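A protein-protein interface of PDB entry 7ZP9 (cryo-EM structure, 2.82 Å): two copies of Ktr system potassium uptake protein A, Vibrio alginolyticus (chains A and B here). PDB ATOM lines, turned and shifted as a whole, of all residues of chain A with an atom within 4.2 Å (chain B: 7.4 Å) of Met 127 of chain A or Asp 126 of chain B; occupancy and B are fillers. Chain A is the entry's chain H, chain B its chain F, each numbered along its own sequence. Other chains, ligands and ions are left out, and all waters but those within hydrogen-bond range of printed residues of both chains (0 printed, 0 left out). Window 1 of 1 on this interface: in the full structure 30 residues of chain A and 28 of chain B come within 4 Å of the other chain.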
ATOM      1  N   PRO A 123      20.372 -27.735  -1.487  1.00  0.00           N
ATOM      2  CA  PRO A 123      20.144 -28.102  -0.077  1.00  0.00           C
ATOM      3  C   PRO A 123      19.902 -26.912   0.835  1.00  0.00           C
ATOM      4  O   PRO A 123      19.031 -26.976   1.706  1.00  0.00           O
ATOM      5  CB  PRO A 123      21.455 -28.793   0.309  1.00  0.00           C
ATOM      6  CG  PRO A 123      21.959 -29.385  -0.961  1.00  0.00           C
ATOM      7  CD  PRO A 123      21.623 -28.389  -2.026  1.00  0.00           C
ATOM      8  N   GLU A 124      20.644 -25.818   0.657  1.00  0.00           N
ATOM      9  CA  GLU A 124      20.511 -24.685   1.568  1.00  0.00           C
ATOM     10  C   GLU A 124      19.216 -23.921   1.321  1.00  0.00           C
ATOM     11  O   GLU A 124      18.503 -23.562   2.264  1.00  0.00           O
ATOM     12  CB  GLU A 124      21.718 -23.759   1.431  1.00  0.00           C
ATOM     13  CG  GLU A 124      23.041 -24.411   1.790  1.00  0.00           C
ATOM     14  CD  GLU A 124      23.378 -24.284   3.261  1.00  0.00           C
ATOM     15  OE1 GLU A 124      24.574 -24.150   3.588  1.00  0.00           O
ATOM     16  OE2 GLU A 124      22.446 -24.318   4.091  1.00  0.00           O
ATOM     17  N   ARG A 125      18.898 -23.658   0.054  1.00  0.00           N
ATOM     18  CA  ARG A 125      17.727 -22.848  -0.264  1.00  0.00           C
ATOM     19  C   ARG A 125      16.433 -23.618  -0.025  1.00  0.00           C
ATOM     20  O   ARG A 125      15.493 -23.094   0.588  1.00  0.00           O
ATOM     21  CB  ARG A 125      17.824 -22.364  -1.712  1.00  0.00           C
ATOM     22  CG  ARG A 125      16.811 -21.310  -2.106  1.00  0.00           C
ATOM     23  CD  ARG A 125      15.750 -21.884  -3.019  1.00  0.00           C
ATOM     24  NE  ARG A 125      16.303 -22.338  -4.289  1.00  0.00           N
ATOM     25  CZ  ARG A 125      15.682 -23.161  -5.121  1.00  0.00           C
ATOM     26  NH1 ARG A 125      14.489 -23.658  -4.841  1.00  0.00           N
ATOM     27  NH2 ARG A 125      16.275 -23.499  -6.263  1.00  0.00           N
ATOM     28  N   ASP A 126      16.371 -24.866  -0.491  1.00  0.00           N
ATOM     29  CA  ASP A 126      15.157 -25.659  -0.325  1.00  0.00           C
ATOM     30  C   ASP A 126      14.892 -25.971   1.141  1.00  0.00           C
ATOM     31  O   ASP A 126      13.745 -25.906   1.598  1.00  0.00           O
ATOM     32  CB  ASP A 126      15.260 -26.943  -1.142  1.00  0.00           C
ATOM     33  CG  ASP A 126      15.213 -26.687  -2.633  1.00  0.00           C
ATOM     34  OD1 ASP A 126      14.765 -25.592  -3.031  1.00  0.00           O
ATOM     35  OD2 ASP A 126      15.621 -27.578  -3.405  1.00  0.00           O
ATOM     36  N   MET A 127      15.936 -26.309   1.898  1.00  0.00           N
ATOM     37  CA  MET A 127      15.743 -26.566   3.320  1.00  0.00           C
ATOM     38  C   MET A 127      15.361 -25.282   4.042  1.00  0.00           C
ATOM     39  O   MET A 127      14.619 -25.312   5.028  1.00  0.00           O
ATOM     40  CB  MET A 127      17.009 -27.170   3.924  1.00  0.00           C
ATOM     41  CG  MET A 127      16.874 -27.641   5.357  1.00  0.00           C
ATOM     42  SD  MET A 127      15.729 -29.036   5.425  1.00  0.00           S
ATOM     43  CE  MET A 127      15.169 -28.973   7.120  1.00  0.00           C
ATOM     44  N   GLY A 128      15.862 -24.141   3.562  1.00  0.00           N
ATOM     45  CA  GLY A 128      15.441 -22.866   4.118  1.00  0.00           C
ATOM     46  C   GLY A 128      13.959 -22.616   3.927  1.00  0.00           C
ATOM     47  O   GLY A 128      13.257 -22.218   4.860  1.00  0.00           O
ATOM     48  N   ILE A 129      13.459 -22.862   2.715  1.00  0.00           N
ATOM     49  CA  ILE A 129      12.022 -22.743   2.475  1.00  0.00           C
ATOM     50  C   ILE A 129      11.251 -23.709   3.363  1.00  0.00           C
ATOM     51  O   ILE A 129      10.205 -23.361   3.929  1.00  0.00           O
ATOM     52  CB  ILE A 129      11.705 -22.969   0.985  1.00  0.00           C
ATOM     53  CG1 ILE A 129      12.295 -21.849   0.134  1.00  0.00           C
ATOM     54  CG2 ILE A 129      10.209 -23.072   0.765  1.00  0.00           C
ATOM     55  CD1 ILE A 129      12.747 -22.303  -1.224  1.00  0.00           C
ATOM     56  N   ARG A 130      11.748 -24.940   3.497  1.00  0.00           N
ATOM     57  CA  ARG A 130      11.022 -25.937   4.272  1.00  0.00           C
ATOM     58  C   ARG A 130      10.945 -25.551   5.745  1.00  0.00           C
ATOM     59  O   ARG A 130       9.882 -25.662   6.363  1.00  0.00           O
ATOM     60  CB  ARG A 130      11.670 -27.310   4.106  1.00  0.00           C
ATOM     61  CG  ARG A 130      10.918 -28.418   4.817  1.00  0.00           C
ATOM     62  CD  ARG A 130      11.560 -29.772   4.584  1.00  0.00           C
ATOM     63  NE  ARG A 130      10.810 -30.842   5.231  1.00  0.00           N
ATOM     64  CZ  ARG A 130      11.015 -31.264   6.470  1.00  0.00           C
ATOM     65  NH1 ARG A 130      11.961 -30.740   7.232  1.00  0.00           N
ATOM     66  NH2 ARG A 130      10.249 -32.236   6.958  1.00  0.00           N
ATOM     67  N   VAL A 131      12.052 -25.079   6.325  1.00  0.00           N
ATOM     68  CA  VAL A 131      12.012 -24.674   7.727  1.00  0.00           C
ATOM     69  C   VAL A 131      11.175 -23.415   7.900  1.00  0.00           C
ATOM     70  O   VAL A 131      10.510 -23.247   8.927  1.00  0.00           O
ATOM     71  CB  VAL A 131      13.428 -24.491   8.311  1.00  0.00           C
ATOM     72  CG1 VAL A 131      14.219 -25.774   8.201  1.00  0.00           C
ATOM     73  CG2 VAL A 131      14.158 -23.356   7.635  1.00  0.00           C
ATOM     74  N   PHE B  16      20.759 -19.936   2.922  1.00  0.00           N
ATOM     75  CA  PHE B  16      19.719 -20.527   3.755  1.00  0.00           C
ATOM     76  C   PHE B  16      18.894 -19.449   4.448  1.00  0.00           C
ATOM     77  O   PHE B  16      17.656 -19.507   4.467  1.00  0.00           O
ATOM     78  CB  PHE B  16      20.373 -21.464   4.770  1.00  0.00           C
ATOM     79  CG  PHE B  16      19.418 -22.088   5.731  1.00  0.00           C
ATOM     80  CD1 PHE B  16      18.799 -23.286   5.431  1.00  0.00           C
ATOM     81  CD2 PHE B  16      19.147 -21.485   6.941  1.00  0.00           C
ATOM     82  CE1 PHE B  16      17.928 -23.864   6.319  1.00  0.00           C
ATOM     83  CE2 PHE B  16      18.273 -22.055   7.821  1.00  0.00           C
ATOM     84  CZ  PHE B  16      17.664 -23.248   7.516  1.00  0.00           C
ATOM     85  N   ALA B  19      16.590 -17.507   2.241  1.00  0.00           N
ATOM     86  CA  ALA B  19      15.485 -18.365   1.776  1.00  0.00           C
ATOM     87  C   ALA B  19      14.405 -18.418   2.846  1.00  0.00           C
ATOM     88  O   ALA B  19      13.226 -18.423   2.480  1.00  0.00           O
ATOM     89  CB  ALA B  19      16.020 -19.728   1.465  1.00  0.00           C
ATOM     90  N   VAL B  20      14.801 -18.452   4.116  1.00  0.00           N
ATOM     91  CA  VAL B  20      13.822 -18.461   5.237  1.00  0.00           C
ATOM     92  C   VAL B  20      13.153 -17.088   5.297  1.00  0.00           C
ATOM     93  O   VAL B  20      11.955 -17.034   5.588  1.00  0.00           O
ATOM     94  CB  VAL B  20      14.493 -18.828   6.573  1.00  0.00           C
ATOM     95  CG1 VAL B  20      13.478 -18.989   7.689  1.00  0.00           C
ATOM     96  CG2 VAL B  20      15.355 -20.070   6.449  1.00  0.00           C
ATOM     97  N   LYS B 102      20.949 -23.530  12.573  1.00  0.00           N
ATOM     98  CA  LYS B 102      21.456 -24.327  11.466  1.00  0.00           C
ATOM     99  C   LYS B 102      22.851 -24.837  11.801  1.00  0.00           C
ATOM    100  O   LYS B 102      23.723 -24.060  12.201  1.00  0.00           O
ATOM    101  CB  LYS B 102      21.496 -23.512  10.174  1.00  0.00           C
ATOM    102  CG  LYS B 102      22.020 -24.295   8.983  1.00  0.00           C
ATOM    103  CD  LYS B 102      21.990 -23.473   7.713  1.00  0.00           C
ATOM    104  CE  LYS B 102      23.112 -22.454   7.683  1.00  0.00           C
ATOM    105  NZ  LYS B 102      24.434 -23.102   7.485  1.00  0.00           N
ATOM    106  N   ILE B 120      17.541 -28.050  15.743  1.00  0.00           N
ATOM    107  CA  ILE B 120      18.790 -28.053  14.993  1.00  0.00           C
ATOM    108  C   ILE B 120      18.481 -28.495  13.573  1.00  0.00           C
ATOM    109  O   ILE B 120      17.912 -29.573  13.361  1.00  0.00           O
ATOM    110  CB  ILE B 120      19.843 -28.969  15.638  1.00  0.00           C
ATOM    111  CG1 ILE B 120      20.261 -28.435  17.008  1.00  0.00           C
ATOM    112  CG2 ILE B 120      21.051 -29.110  14.733  1.00  0.00           C
ATOM    113  CD1 ILE B 120      19.501 -29.040  18.157  1.00  0.00           C
ATOM    114  N   ILE B 121      18.855 -27.669  12.601  1.00  0.00           N
ATOM    115  CA  ILE B 121      18.603 -27.939  11.193  1.00  0.00           C
ATOM    116  C   ILE B 121      19.932 -28.270  10.532  1.00  0.00           C
ATOM    117  O   ILE B 121      20.868 -27.462  10.565  1.00  0.00           O
ATOM    118  CB  ILE B 121      17.923 -26.754  10.491  1.00  0.00           C
ATOM    119  CG1 ILE B 121      16.536 -26.489  11.080  1.00  0.00           C
ATOM    120  CG2 ILE B 121      17.822 -27.010   8.999  1.00  0.00           C
ATOM    121  CD1 ILE B 121      16.524 -25.500  12.221  1.00  0.00           C
ATOM    122  N   MET B 122      20.015 -29.456   9.934  1.00  0.00           N
ATOM    123  CA  MET B 122      21.171 -29.827   9.134  1.00  0.00           C
ATOM    124  C   MET B 122      20.720 -29.917   7.686  1.00  0.00           C
ATOM    125  O   MET B 122      20.144 -30.937   7.283  1.00  0.00           O
ATOM    126  CB  MET B 122      21.762 -31.157   9.605  1.00  0.00           C
ATOM    127  CG  MET B 122      22.369 -31.092  10.996  1.00  0.00           C
ATOM    128  SD  MET B 122      22.991 -32.678  11.581  1.00  0.00           S
ATOM    129  CE  MET B 122      24.420 -32.886  10.522  1.00  0.00           C
ATOM    130  N   PRO B 123      20.947 -28.884   6.868  1.00  0.00           N
ATOM    131  CA  PRO B 123      20.328 -28.860   5.533  1.00  0.00           C
ATOM    132  C   PRO B 123      20.740 -30.009   4.629  1.00  0.00           C
ATOM    133  O   PRO B 123      19.925 -30.460   3.818  1.00  0.00           O
ATOM    134  CB  PRO B 123      20.772 -27.500   4.976  1.00  0.00           C
ATOM    135  CG  PRO B 123      20.934 -26.638   6.175  1.00  0.00           C
ATOM    136  CD  PRO B 123      21.510 -27.526   7.232  1.00  0.00           C
ATOM    137  N   GLU B 124      21.976 -30.498   4.730  1.00  0.00           N
ATOM    138  CA  GLU B 124      22.407 -31.575   3.843  1.00  0.00           C
ATOM    139  C   GLU B 124      21.726 -32.893   4.194  1.00  0.00           C
ATOM    140  O   GLU B 124      21.236 -33.603   3.310  1.00  0.00           O
ATOM    141  CB  GLU B 124      23.927 -31.721   3.891  1.00  0.00           C
ATOM    142  CG  GLU B 124      24.695 -30.549   3.293  1.00  0.00           C
ATOM    143  CD  GLU B 124      24.704 -30.537   1.774  1.00  0.00           C
ATOM    144  OE1 GLU B 124      23.750 -31.042   1.152  1.00  0.00           O
ATOM    145  OE2 GLU B 124      25.676 -30.010   1.196  1.00  0.00           O
ATOM    146  N   ARG B 125      21.692 -33.240   5.480  1.00  0.00           N
ATOM    147  CA  ARG B 125      21.094 -34.509   5.882  1.00  0.00           C
ATOM    148  C   ARG B 125      19.577 -34.485   5.726  1.00  0.00           C
ATOM    149  O   ARG B 125      18.986 -35.426   5.182  1.00  0.00           O
ATOM    150  CB  ARG B 125      21.484 -34.834   7.324  1.00  0.00           C
ATOM    151  CG  ARG B 125      20.677 -35.954   7.953  1.00  0.00           C
ATOM    152  CD  ARG B 125      21.033 -36.133   9.416  1.00  0.00           C
ATOM    153  NE  ARG B 125      20.673 -34.972  10.220  1.00  0.00           N
ATOM    154  CZ  ARG B 125      19.647 -34.932  11.058  1.00  0.00           C
ATOM    155  NH1 ARG B 125      18.853 -35.976  11.228  1.00  0.00           N
ATOM    156  NH2 ARG B 125      19.414 -33.819  11.747  1.00  0.00           N
ATOM    157  N   ASP B 126      18.930 -33.418   6.199  1.00  0.00           N
ATOM    158  CA  ASP B 126      17.474 -33.344   6.133  1.00  0.00           C
ATOM    159  C   ASP B 126      16.984 -33.296   4.693  1.00  0.00           C
ATOM    160  O   ASP B 126      16.031 -33.999   4.328  1.00  0.00           O
ATOM    161  CB  ASP B 126      16.980 -32.128   6.912  1.00  0.00           C
ATOM    162  CG  ASP B 126      17.392 -32.165   8.369  1.00  0.00           C
ATOM    163  OD1 ASP B 126      17.902 -33.214   8.814  1.00  0.00           O
ATOM    164  OD2 ASP B 126      17.211 -31.147   9.070  1.00  0.00           O
ATOM    165  N   MET B 127      17.622 -32.477   3.854  1.00  0.00           N
ATOM    166  CA  MET B 127      17.252 -32.463   2.446  1.00  0.00           C
ATOM    167  C   MET B 127      17.594 -33.779   1.771  1.00  0.00           C
ATOM    168  O   MET B 127      16.899 -34.187   0.842  1.00  0.00           O
ATOM    169  CB  MET B 127      17.918 -31.301   1.716  1.00  0.00           C
ATOM    170  CG  MET B 127      17.068 -30.760   0.588  1.00  0.00           C
ATOM    171  SD  MET B 127      15.518 -30.070   1.191  1.00  0.00           S
ATOM    172  CE  MET B 127      14.479 -30.289  -0.249  1.00  0.00           C
ATOM    173  N   GLY B 128      18.646 -34.461   2.223  1.00  0.00           N
ATOM    174  CA  GLY B 128      18.917 -35.790   1.702  1.00  0.00           C
ATOM    175  C   GLY B 128      17.778 -36.755   1.968  1.00  0.00           C
ATOM    176  O   GLY B 128      17.326 -37.463   1.063  1.00  0.00           O
ATOM    177  N   ILE B 129      17.279 -36.771   3.205  1.00  0.00           N
ATOM    178  CA  ILE B 129      16.153 -37.638   3.543  1.00  0.00           C
ATOM    179  C   ILE B 129      14.924 -37.265   2.726  1.00  0.00           C
ATOM    180  O   ILE B 129      14.230 -38.135   2.184  1.00  0.00           O
ATOM    181  CB  ILE B 129      15.861 -37.577   5.053  1.00  0.00           C
ATOM    182  CG1 ILE B 129      17.040 -38.130   5.853  1.00  0.00           C
ATOM    183  CG2 ILE B 129      14.591 -38.337   5.382  1.00  0.00           C
ATOM    184  CD1 ILE B 129      17.284 -37.403   7.149  1.00  0.00           C
ATOM    185  N   ARG B 130      14.636 -35.966   2.617  1.00  0.00           N
ATOM    186  CA  ARG B 130      13.425 -35.549   1.917  1.00  0.00           C
ATOM    187  C   ARG B 130      13.518 -35.841   0.424  1.00  0.00           C
ATOM    188  O   ARG B 130      12.525 -36.227  -0.203  1.00  0.00           O
ATOM    189  CB  ARG B 130      13.158 -34.065   2.164  1.00  0.00           C
ATOM    190  CG  ARG B 130      11.862 -33.575   1.550  1.00  0.00           C
ATOM    191  CD  ARG B 130      11.589 -32.125   1.900  1.00  0.00           C
ATOM    192  NE  ARG B 130      10.384 -31.629   1.247  1.00  0.00           N
ATOM    193  CZ  ARG B 130       9.162 -31.753   1.745  1.00  0.00           C
ATOM    194  NH1 ARG B 130       8.945 -32.360   2.901  1.00  0.00           N
ATOM    195  NH2 ARG B 130       8.131 -31.260   1.065  1.00  0.00           N
ATOM    196  N   VAL B 131      14.705 -35.684  -0.162  1.00  0.00           N
ATOM    197  CA  VAL B 131      14.891 -35.980  -1.577  1.00  0.00           C
ATOM    198  C   VAL B 131      14.774 -37.476  -1.830  1.00  0.00           C
ATOM    199  O   VAL B 131      14.212 -37.904  -2.843  1.00  0.00           O
ATOM    200  CB  VAL B 131      16.240 -35.418  -2.061  1.00  0.00           C
ATOM    201  CG1 VAL B 131      16.651 -36.052  -3.378  1.00  0.00           C
ATOM    202  CG2 VAL B 131      16.152 -33.915  -2.205  1.00  0.00           C
ATOM    203  N   ALA B 132      15.297 -38.298  -0.917  1.00  0.00           N
ATOM    204  CA  ALA B 132      15.110 -39.738  -1.057  1.00  0.00           C
ATOM    205  C   ALA B 132      13.633 -40.107  -0.982  1.00  0.00           C
ATOM    206  O   ALA B 132      13.155 -40.946  -1.755  1.00  0.00           O
ATOM    207  CB  ALA B 132      15.906 -40.477   0.014  1.00  0.00           C
ATOM    208  N   ARG B 133      12.894 -39.479  -0.067  1.00  0.00           N
ATOM    209  CA  ARG B 133      11.457 -39.730   0.026  1.00  0.00           C
ATOM    210  C   ARG B 133      10.736 -39.304  -1.248  1.00  0.00           C
ATOM    211  O   ARG B 133       9.794 -39.972  -1.689  1.00  0.00           O
ATOM    212  CB  ARG B 133      10.880 -39.008   1.241  1.00  0.00           C
ATOM    213  CG  ARG B 133      11.360 -39.567   2.563  1.00  0.00           C
ATOM    214  CD  ARG B 133      10.762 -38.815   3.733  1.00  0.00           C
ATOM    215  NE  ARG B 133      11.237 -39.337   5.007  1.00  0.00           N
ATOM    216  CZ  ARG B 133      10.918 -38.831   6.189  1.00  0.00           C
ATOM    217  NH1 ARG B 133      10.143 -37.765   6.297  1.00  0.00           N
ATOM    218  NH2 ARG B 133      11.389 -39.408   7.291  1.00  0.00           N
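NH1 of Arg 130 of chain B lies close to NE of Arg 130 of chain A (3.3 Å).
The guanidinium group (NH1) of Arg 125 of chain A is in salt-bridge range of the side-chain carboxylate (OD1) of Asp 126 of chain A (2.7 Å).
The side-chain carboxylate of Asp 126 of chain B lies within hydrogen-bond range of the backbone NH of Met 122 of chain B (3.4 Å).
The side-chain carboxylate (OD1) of Asp 126 of chain B is in salt-bridge range of the guanidinium group (NH2) of Arg 125 of chain B (3.4 Å).
Pro 123 of chain A touches Pro 123 of chain B (O to CB, 3.7 Å).
Ala 19 of chain B touches Arg 125 of chain A (CB to O, 3.5 Å).
C of Met 127 of chain A touches CE1 of Phe 16 of chain B, 3.7 Å away.
Ile 121 of chain B touches Met 127 of chain A (CG2 to CE, 3.8 Å).
Met 127 of chain A touches Pro 123 of chain B (CG to CA, 3.7 Å).
Asp 126 of chain B touches Met 127 of chain A.
N of Met 127 of chain A touches SD of Met 127 of chain B, 3.8 Å away.
N of Gly 128 of chain A touches CE1 of Phe 16 of chain B, at 3.5 Å.
Gly 128 of chain A touches Val 20 of chain B (O to CG2, 3.4 Å).
Val 131 of chain A touches Ile 121 of chain B.
Of chain B, only Phe 16 (3.7 Å), Ile 121 (3.8 Å), Pro 123 (3.7 Å), Asp 126 (3.6 Å) and Met 127 (3.8 Å) come within 4 Å of Met 127 of chain A.
Printed residues of chain B within 4 Å of Val 131 of chain A: Phe 16, Val 20 and Ile 121.
Of the printed residues of chain B, Pro 123 of chain A touches Pro 123 (3.7 Å) and Glu 124 (3.2 Å).
Of the printed residues of chain A, Ala 19 of chain B touches Arg 125.
Printed residues of chain A within 4 Å of Phe 16 of chain B: Glu 124, Met 127, Gly 128 and Val 131.
The nearest residue of chain B that does not touch Met 127 of chain A is Met 122 of chain B (5.0 Å).
Hydrophobic or aromatic side chains of chain A within 4 Å of the printed part of chain B: Pro 123, Met 127 and Val 131.
Hydrophobic or aromatic side chains of chain B that line the printed part of chain A: Phe 16, Ala 19, Val 20, Ile 121, Pro 123 and Met 127.
Among the printed residues, 18 pairs touch across the chains.
Among the printed residues, no Asp or Glu carboxylate lies within 4 Å of a Lys or Arg side-chain nitrogen of the other chain.
Pro 123 of chain A touches its own counterpart, Pro 123 of chain B.
Met 127 of chain A touches Pro 123 of chain B, but with the chains exchanged Pro 123 of chain A does not touch Met 127 of chain B (4.1 Å).
Met 127 of chain A touches its own counterpart, Met 127 of chain B.
Arg 130 of chain A touches its own counterpart, Arg 130 of chain B.
Positions printed for both chains: 123, 124, 125, 126, 127, 128, 129, 130 and 131.
Of the 18 pairs that touch across the chains among the printed residues, 7 have their exchanged pair printed and touching as well.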
